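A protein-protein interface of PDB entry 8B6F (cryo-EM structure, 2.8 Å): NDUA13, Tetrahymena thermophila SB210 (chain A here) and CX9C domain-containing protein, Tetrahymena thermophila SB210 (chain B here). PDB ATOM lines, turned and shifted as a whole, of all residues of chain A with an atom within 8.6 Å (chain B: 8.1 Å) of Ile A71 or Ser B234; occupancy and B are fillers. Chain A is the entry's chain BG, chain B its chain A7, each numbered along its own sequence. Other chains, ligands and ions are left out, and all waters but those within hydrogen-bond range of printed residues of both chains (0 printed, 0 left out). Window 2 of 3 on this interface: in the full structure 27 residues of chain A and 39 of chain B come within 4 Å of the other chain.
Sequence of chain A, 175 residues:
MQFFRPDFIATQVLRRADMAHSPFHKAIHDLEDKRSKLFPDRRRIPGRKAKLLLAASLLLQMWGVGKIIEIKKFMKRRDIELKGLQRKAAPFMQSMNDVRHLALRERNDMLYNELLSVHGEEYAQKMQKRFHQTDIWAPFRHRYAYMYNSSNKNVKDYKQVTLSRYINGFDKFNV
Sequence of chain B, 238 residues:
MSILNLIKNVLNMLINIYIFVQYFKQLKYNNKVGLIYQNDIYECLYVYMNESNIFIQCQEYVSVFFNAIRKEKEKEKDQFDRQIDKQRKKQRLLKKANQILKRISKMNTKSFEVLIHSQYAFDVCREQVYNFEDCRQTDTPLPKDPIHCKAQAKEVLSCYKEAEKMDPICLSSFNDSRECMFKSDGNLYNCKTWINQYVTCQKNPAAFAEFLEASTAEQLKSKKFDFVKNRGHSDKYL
Ser B234 touches just these residues of chain A: Ile A71, Met A75 and Arg A78. Printed residues of chain A within 4 Å of His B233: Arg A78 (3.0 Å). Of the printed residues of chain B, Arg A78 touches His B233 (3.0 Å), Ser B234 (2.5 Å) and Asp B235 (3.4 Å). The nearest residue of chain B that does not touch Ile A71 is Lys B236 (7.1 Å). The nearest printed residue of chain A that does not touch His B233 is Phe A74 (4.9 Å).
Printed residues of chain A that touch a printed residue of chain B: Ile A71, Met A75, Arg A78 and Asp A79. Of the 9 printed residues of chain B, 5 touch a printed residue of chain A. Hydrophobic or aromatic side chains of chain B that line the printed part of chain A: Leu B238. Among the printed residues, 8 pairs touch across the chains. Among the printed residues, Asp or Glu carboxylates within 4 Å of a Lys or Arg side-chain nitrogen of the other chain: Asp A79 with Lys B236 (3.2 Å).
O of Met A75 lies close to OD1 of Asp A79, at 2.6 Å. The side-chain carboxylate (OD2) of Asp B235 is in hydrogen-bond range of the side-chain amide nitrogen (ND2) of Asn B190 (3.4 Å). The backbone NH (N) of Tyr B237 lies within hydrogen-bond range of the side-chain carboxylate (OD1) of Asp B235 (2.8 Å).
The guanidinium group (NH2) of Arg A78 is in hydrogen-bond range of the backbone carbonyl oxygen (O) of His B233 (3.0 Å). The backbone carbonyl oxygen (O) of Ser B234 sits at hydrogen-bond distance from the guanidinium group (NH2) of Arg A78 (2.5 Å). The side-chain carboxylate of Asp A79 is in salt-bridge range of the side-chain amino group of Lys B236. OD1 of Asp A79 lies close to OXT of Leu B238 (2.6 Å). The guanidinium group of Arg A78 sits close to the backbone NH of Asp B235, 3.5 Å away.
Among the printed residues, pairs that only touch across the chains: Ile A71 with Ser B234, Met A75 with Ser B234 and Met A75 with Lys B236.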
ATOM      1  N   GLY A  64      -1.991  -9.091   3.804  1.00  0.00           N
ATOM      2  CA  GLY A  64      -2.958  -8.079   4.194  1.00  0.00           C
ATOM      3  C   GLY A  64      -2.690  -7.513   5.574  1.00  0.00           C
ATOM      4  O   GLY A  64      -2.835  -6.309   5.798  1.00  0.00           O
ATOM      5  N   VAL A  65      -2.289  -8.365   6.519  1.00  0.00           N
ATOM      6  CA  VAL A  65      -1.915  -7.871   7.840  1.00  0.00           C
ATOM      7  C   VAL A  65      -0.714  -6.945   7.730  1.00  0.00           C
ATOM      8  O   VAL A  65      -0.670  -5.883   8.361  1.00  0.00           O
ATOM      9  CB  VAL A  65      -1.646  -9.046   8.797  1.00  0.00           C
ATOM     10  CG1 VAL A  65      -1.076  -8.547  10.119  1.00  0.00           C
ATOM     11  CG2 VAL A  65      -2.921  -9.826   9.046  1.00  0.00           C
ATOM     12  N   GLY A  66       0.277  -7.326   6.923  1.00  0.00           N
ATOM     13  CA  GLY A  66       1.417  -6.452   6.711  1.00  0.00           C
ATOM     14  C   GLY A  66       1.016  -5.116   6.122  1.00  0.00           C
ATOM     15  O   GLY A  66       1.532  -4.070   6.521  1.00  0.00           O
ATOM     16  N   LYS A  67       0.097  -5.132   5.156  1.00  0.00           N
ATOM     17  CA  LYS A  67      -0.356  -3.887   4.544  1.00  0.00           C
ATOM     18  C   LYS A  67      -1.092  -3.010   5.550  1.00  0.00           C
ATOM     19  O   LYS A  67      -0.906  -1.789   5.566  1.00  0.00           O
ATOM     20  CB  LYS A  67      -1.244  -4.196   3.340  1.00  0.00           C
ATOM     21  CG  LYS A  67      -1.669  -2.970   2.539  1.00  0.00           C
ATOM     22  CD  LYS A  67      -0.488  -2.223   1.928  1.00  0.00           C
ATOM     23  CE  LYS A  67       0.302  -3.094   0.965  1.00  0.00           C
ATOM     24  NZ  LYS A  67       1.341  -2.311   0.244  1.00  0.00           N
ATOM     25  N   ILE A  68      -1.928  -3.611   6.398  1.00  0.00           N
ATOM     26  CA  ILE A  68      -2.643  -2.838   7.410  1.00  0.00           C
ATOM     27  C   ILE A  68      -1.662  -2.231   8.404  1.00  0.00           C
ATOM     28  O   ILE A  68      -1.837  -1.092   8.852  1.00  0.00           O
ATOM     29  CB  ILE A  68      -3.693  -3.719   8.115  1.00  0.00           C
ATOM     30  CG1 ILE A  68      -4.790  -4.152   7.135  1.00  0.00           C
ATOM     31  CG2 ILE A  68      -4.306  -2.989   9.306  1.00  0.00           C
ATOM     32  CD1 ILE A  68      -5.604  -3.020   6.545  1.00  0.00           C
ATOM     33  N   ILE A  69      -0.622  -2.979   8.774  1.00  0.00           N
ATOM     34  CA  ILE A  69       0.392  -2.430   9.666  1.00  0.00           C
ATOM     35  C   ILE A  69       1.125  -1.284   8.982  1.00  0.00           C
ATOM     36  O   ILE A  69       1.474  -0.286   9.620  1.00  0.00           O
ATOM     37  CB  ILE A  69       1.360  -3.535  10.127  1.00  0.00           C
ATOM     38  CG1 ILE A  69       0.626  -4.578  10.977  1.00  0.00           C
ATOM     39  CG2 ILE A  69       2.530  -2.941  10.909  1.00  0.00           C
ATOM     40  CD1 ILE A  69       0.028  -4.047  12.263  1.00  0.00           C
ATOM     41  N   GLU A  70       1.374  -1.409   7.678  1.00  0.00           N
ATOM     42  CA  GLU A  70       1.992  -0.313   6.942  1.00  0.00           C
ATOM     43  C   GLU A  70       1.118   0.932   6.995  1.00  0.00           C
ATOM     44  O   GLU A  70       1.617   2.044   7.200  1.00  0.00           O
ATOM     45  CB  GLU A  70       2.239  -0.738   5.494  1.00  0.00           C
ATOM     46  CG  GLU A  70       2.964   0.294   4.641  1.00  0.00           C
ATOM     47  CD  GLU A  70       4.442   0.397   4.967  1.00  0.00           C
ATOM     48  OE1 GLU A  70       5.035  -0.621   5.384  1.00  0.00           O
ATOM     49  OE2 GLU A  70       5.011   1.497   4.806  1.00  0.00           O
ATOM     50  N   ILE A  71      -0.191   0.767   6.795  1.00  0.00           N
ATOM     51  CA  ILE A  71      -1.106   1.903   6.855  1.00  0.00           C
ATOM     52  C   ILE A  71      -1.099   2.519   8.248  1.00  0.00           C
ATOM     53  O   ILE A  71      -1.058   3.745   8.399  1.00  0.00           O
ATOM     54  CB  ILE A  71      -2.523   1.468   6.439  1.00  0.00           C
ATOM     55  CG1 ILE A  71      -2.524   0.988   4.988  1.00  0.00           C
ATOM     56  CG2 ILE A  71      -3.508   2.617   6.604  1.00  0.00           C
ATOM     57  CD1 ILE A  71      -3.800   0.290   4.572  1.00  0.00           C
ATOM     58  N   LYS A  72      -1.140   1.681   9.286  1.00  0.00           N
ATOM     59  CA  LYS A  72      -1.132   2.197  10.651  1.00  0.00           C
ATOM     60  C   LYS A  72       0.142   2.974  10.945  1.00  0.00           C
ATOM     61  O   LYS A  72       0.100   4.028  11.588  1.00  0.00           O
ATOM     62  CB  LYS A  72      -1.294   1.048  11.646  1.00  0.00           C
ATOM     63  CG  LYS A  72      -2.714   0.523  11.771  1.00  0.00           C
ATOM     64  CD  LYS A  72      -2.817  -0.512  12.883  1.00  0.00           C
ATOM     65  CE  LYS A  72      -4.264  -0.863  13.191  1.00  0.00           C
ATOM     66  NZ  LYS A  72      -4.943  -1.509  12.038  1.00  0.00           N
ATOM     67  N   LYS A  73       1.287   2.468  10.489  1.00  0.00           N
ATOM     68  CA  LYS A  73       2.544   3.160  10.745  1.00  0.00           C
ATOM     69  C   LYS A  73       2.638   4.467   9.971  1.00  0.00           C
ATOM     70  O   LYS A  73       3.216   5.438  10.470  1.00  0.00           O
ATOM     71  CB  LYS A  73       3.719   2.245  10.409  1.00  0.00           C
ATOM     72  CG  LYS A  73       3.792   1.009  11.293  1.00  0.00           C
ATOM     73  CD  LYS A  73       4.175   1.356  12.722  1.00  0.00           C
ATOM     74  CE  LYS A  73       4.310   0.102  13.567  1.00  0.00           C
ATOM     75  NZ  LYS A  73       4.719   0.415  14.963  1.00  0.00           N
ATOM     76  N   PHE A  74       2.088   4.516   8.755  1.00  0.00           N
ATOM     77  CA  PHE A  74       2.011   5.786   8.040  1.00  0.00           C
ATOM     78  C   PHE A  74       1.133   6.777   8.791  1.00  0.00           C
ATOM     79  O   PHE A  74       1.472   7.960   8.902  1.00  0.00           O
ATOM     80  CB  PHE A  74       1.479   5.555   6.626  1.00  0.00           C
ATOM     81  CG  PHE A  74       1.445   6.795   5.781  1.00  0.00           C
ATOM     82  CD1 PHE A  74       2.595   7.261   5.166  1.00  0.00           C
ATOM     83  CD2 PHE A  74       0.260   7.486   5.589  1.00  0.00           C
ATOM     84  CE1 PHE A  74       2.565   8.399   4.381  1.00  0.00           C
ATOM     85  CE2 PHE A  74       0.224   8.623   4.807  1.00  0.00           C
ATOM     86  CZ  PHE A  74       1.378   9.082   4.202  1.00  0.00           C
ATOM     87  N   MET A  75      -0.003   6.313   9.313  1.00  0.00           N
ATOM     88  CA  MET A  75      -0.857   7.178  10.118  1.00  0.00           C
ATOM     89  C   MET A  75      -0.105   7.706  11.332  1.00  0.00           C
ATOM     90  O   MET A  75      -0.219   8.886  11.679  1.00  0.00           O
ATOM     91  CB  MET A  75      -2.107   6.417  10.555  1.00  0.00           C
ATOM     92  CG  MET A  75      -3.075   6.110   9.427  1.00  0.00           C
ATOM     93  SD  MET A  75      -4.458   5.095   9.982  1.00  0.00           S
ATOM     94  CE  MET A  75      -5.483   5.079   8.517  1.00  0.00           C
ATOM     95  N   LYS A  76       0.682   6.846  11.980  1.00  0.00           N
ATOM     96  CA  LYS A  76       1.471   7.269  13.131  1.00  0.00           C
ATOM     97  C   LYS A  76       2.539   8.277  12.727  1.00  0.00           C
ATOM     98  O   LYS A  76       2.815   9.228  13.467  1.00  0.00           O
ATOM     99  CB  LYS A  76       2.104   6.051  13.804  1.00  0.00           C
ATOM    100  CG  LYS A  76       2.817   6.367  15.109  1.00  0.00           C
ATOM    101  CD  LYS A  76       3.392   5.115  15.758  1.00  0.00           C
ATOM    102  CE  LYS A  76       2.295   4.185  16.257  1.00  0.00           C
ATOM    103  NZ  LYS A  76       2.852   3.018  16.998  1.00  0.00           N
ATOM    104  N   ARG A  77       3.161   8.080  11.564  1.00  0.00           N
ATOM    105  CA  ARG A  77       4.122   9.060  11.068  1.00  0.00           C
ATOM    106  C   ARG A  77       3.487  10.439  10.951  1.00  0.00           C
ATOM    107  O   ARG A  77       4.081  11.442  11.360  1.00  0.00           O
ATOM    108  CB  ARG A  77       4.679   8.609   9.719  1.00  0.00           C
ATOM    109  CG  ARG A  77       5.733   7.520   9.824  1.00  0.00           C
ATOM    110  CD  ARG A  77       6.386   7.243   8.479  1.00  0.00           C
ATOM    111  NE  ARG A  77       5.586   6.352   7.648  1.00  0.00           N
ATOM    112  CZ  ARG A  77       5.737   5.035   7.594  1.00  0.00           C
ATOM    113  NH1 ARG A  77       6.649   4.412   8.319  1.00  0.00           N
ATOM    114  NH2 ARG A  77       4.952   4.325   6.789  1.00  0.00           N
ATOM    115  N   ARG A  78       2.276  10.511  10.399  1.00  0.00           N
ATOM    116  CA  ARG A  78       1.584  11.791  10.301  1.00  0.00           C
ATOM    117  C   ARG A  78       1.121  12.279  11.666  1.00  0.00           C
ATOM    118  O   ARG A  78       1.057  13.490  11.901  1.00  0.00           O
ATOM    119  CB  ARG A  78       0.405  11.682   9.335  1.00  0.00           C
ATOM    120  CG  ARG A  78       0.828  11.276   7.931  1.00  0.00           C
ATOM    121  CD  ARG A  78      -0.240  11.580   6.897  1.00  0.00           C
ATOM    122  NE  ARG A  78      -1.497  10.903   7.183  1.00  0.00           N
ATOM    123  CZ  ARG A  78      -2.542  10.891   6.368  1.00  0.00           C
ATOM    124  NH1 ARG A  78      -2.510  11.503   5.196  1.00  0.00           N
ATOM    125  NH2 ARG A  78      -3.644  10.248   6.736  1.00  0.00           N
ATOM    126  N   ASP A  79       0.795  11.360  12.577  1.00  0.00           N
ATOM    127  CA  ASP A  79       0.415  11.761  13.926  1.00  0.00           C
ATOM    128  C   ASP A  79       1.556  12.469  14.640  1.00  0.00           C
ATOM    129  O   ASP A  79       1.312  13.316  15.507  1.00  0.00           O
ATOM    130  CB  ASP A  79      -0.021  10.538  14.731  1.00  0.00           C
ATOM    131  CG  ASP A  79      -1.231   9.850  14.135  1.00  0.00           C
ATOM    132  OD1 ASP A  79      -1.780  10.366  13.139  1.00  0.00           O
ATOM    133  OD2 ASP A  79      -1.627   8.786  14.658  1.00  0.00           O
ATOM    134  N   ASN B 190      -4.657  18.395   8.471  1.00  0.00           N
ATOM    135  CA  ASN B 190      -5.288  18.517   7.161  1.00  0.00           C
ATOM    136  C   ASN B 190      -5.189  19.935   6.621  1.00  0.00           C
ATOM    137  O   ASN B 190      -5.149  20.130   5.401  1.00  0.00           O
ATOM    138  CB  ASN B 190      -6.753  18.089   7.238  1.00  0.00           C
ATOM    139  CG  ASN B 190      -6.916  16.614   7.541  1.00  0.00           C
ATOM    140  OD1 ASN B 190      -6.020  15.813   7.281  1.00  0.00           O
ATOM    141  ND2 ASN B 190      -8.069  16.247   8.086  1.00  0.00           N
ATOM    142  N   ARG B 231     -12.296  12.751   1.322  1.00  0.00           N
ATOM    143  CA  ARG B 231     -11.692  12.313   2.576  1.00  0.00           C
ATOM    144  C   ARG B 231     -10.185  12.540   2.585  1.00  0.00           C
ATOM    145  O   ARG B 231      -9.625  12.994   3.591  1.00  0.00           O
ATOM    146  CB  ARG B 231     -12.007  10.837   2.822  1.00  0.00           C
ATOM    147  CG  ARG B 231     -13.457  10.565   3.188  1.00  0.00           C
ATOM    148  CD  ARG B 231     -14.058   9.481   2.315  1.00  0.00           C
ATOM    149  NE  ARG B 231     -14.308   9.960   0.963  1.00  0.00           N
ATOM    150  CZ  ARG B 231     -14.689   9.192  -0.047  1.00  0.00           C
ATOM    151  NH1 ARG B 231     -14.855   7.889   0.099  1.00  0.00           N
ATOM    152  NH2 ARG B 231     -14.909   9.747  -1.236  1.00  0.00           N
ATOM    153  N   GLY B 232      -9.512  12.226   1.483  1.00  0.00           N
ATOM    154  CA  GLY B 232      -8.066  12.322   1.420  1.00  0.00           C
ATOM    155  C   GLY B 232      -7.414  10.965   1.268  1.00  0.00           C
ATOM    156  O   GLY B 232      -7.979  10.071   0.631  1.00  0.00           O
ATOM    157  N   HIS B 233      -6.229  10.793   1.852  1.00  0.00           N
ATOM    158  CA  HIS B 233      -5.479   9.542   1.771  1.00  0.00           C
ATOM    159  C   HIS B 233      -5.233   9.017   3.178  1.00  0.00           C
ATOM    160  O   HIS B 233      -4.448   9.599   3.933  1.00  0.00           O
ATOM    161  CB  HIS B 233      -4.160   9.737   1.026  1.00  0.00           C
ATOM    162  CG  HIS B 233      -4.328  10.058  -0.425  1.00  0.00           C
ATOM    163  ND1 HIS B 233      -4.845  11.257  -0.868  1.00  0.00           N
ATOM    164  CD2 HIS B 233      -4.054   9.335  -1.536  1.00  0.00           C
ATOM    165  CE1 HIS B 233      -4.878  11.258  -2.187  1.00  0.00           C
ATOM    166  NE2 HIS B 233      -4.404  10.104  -2.619  1.00  0.00           N
ATOM    167  N   SER B 234      -5.895   7.915   3.519  1.00  0.00           N
ATOM    168  CA  SER B 234      -5.651   7.207   4.774  1.00  0.00           C
ATOM    169  C   SER B 234      -5.748   8.147   5.973  1.00  0.00           C
ATOM    170  O   SER B 234      -4.913   8.130   6.879  1.00  0.00           O
ATOM    171  CB  SER B 234      -4.291   6.509   4.735  1.00  0.00           C
ATOM    172  OG  SER B 234      -4.021   5.847   5.957  1.00  0.00           O
ATOM    173  N   ASP B 235      -6.790   8.974   5.977  1.00  0.00           N
ATOM    174  CA  ASP B 235      -6.984   9.948   7.046  1.00  0.00           C
ATOM    175  C   ASP B 235      -7.442   9.228   8.307  1.00  0.00           C
ATOM    176  O   ASP B 235      -8.534   8.651   8.341  1.00  0.00           O
ATOM    177  CB  ASP B 235      -7.999  11.004   6.620  1.00  0.00           C
ATOM    178  CG  ASP B 235      -8.126  12.130   7.626  1.00  0.00           C
ATOM    179  OD1 ASP B 235      -7.383  12.119   8.630  1.00  0.00           O
ATOM    180  OD2 ASP B 235      -8.969  13.027   7.416  1.00  0.00           O
ATOM    181  N   LYS B 236      -6.609   9.256   9.345  1.00  0.00           N
ATOM    182  CA  LYS B 236      -6.958   8.669  10.631  1.00  0.00           C
ATOM    183  C   LYS B 236      -7.797   9.604  11.492  1.00  0.00           C
ATOM    184  O   LYS B 236      -8.355   9.159  12.499  1.00  0.00           O
ATOM    185  CB  LYS B 236      -5.687   8.277  11.389  1.00  0.00           C
ATOM    186  CG  LYS B 236      -5.939   7.620  12.739  1.00  0.00           C
ATOM    187  CD  LYS B 236      -4.637   7.239  13.414  1.00  0.00           C
ATOM    188  CE  LYS B 236      -4.885   6.699  14.808  1.00  0.00           C
ATOM    189  NZ  LYS B 236      -3.606   6.401  15.514  1.00  0.00           N
ATOM    190  N   TYR B 237      -7.920  10.875  11.111  1.00  0.00           N
ATOM    191  CA  TYR B 237      -8.570  11.880  11.948  1.00  0.00           C
ATOM    192  C   TYR B 237      -7.882  11.982  13.308  1.00  0.00           C
ATOM    193  O   TYR B 237      -8.524  12.146  14.346  1.00  0.00           O
ATOM    194  CB  TYR B 237     -10.062  11.580  12.103  1.00  0.00           C
ATOM    195  CG  TYR B 237     -10.749  11.368  10.777  1.00  0.00           C
ATOM    196  CD1 TYR B 237     -10.951  12.429   9.904  1.00  0.00           C
ATOM    197  CD2 TYR B 237     -11.186  10.110  10.392  1.00  0.00           C
ATOM    198  CE1 TYR B 237     -11.575  12.242   8.685  1.00  0.00           C
ATOM    199  CE2 TYR B 237     -11.811   9.912   9.176  1.00  0.00           C
ATOM    200  CZ  TYR B 237     -12.003  10.983   8.327  1.00  0.00           C
ATOM    201  OH  TYR B 237     -12.623  10.795   7.115  1.00  0.00           O
ATOM    202  N   LEU B 238      -6.557  11.880  13.288  1.00  0.00           N
ATOM    203  CA  LEU B 238      -5.734  11.980  14.485  1.00  0.00           C
ATOM    204  C   LEU B 238      -4.276  11.970  14.048  1.00  0.00           C
ATOM    205  O   LEU B 238      -3.358  12.159  14.842  1.00  0.00           O
ATOM    206  CB  LEU B 238      -6.019  10.833  15.460  1.00  0.00           C
ATOM    207  CG  LEU B 238      -5.023  10.683  16.621  1.00  0.00           C
ATOM    208  CD1 LEU B 238      -5.739  10.198  17.858  1.00  0.00           C
ATOM    209  CD2 LEU B 238      -3.899   9.720  16.305  1.00  0.00           C
ATOM    210  OXT LEU B 238      -3.982  11.781  12.868  1.00  0.00           O
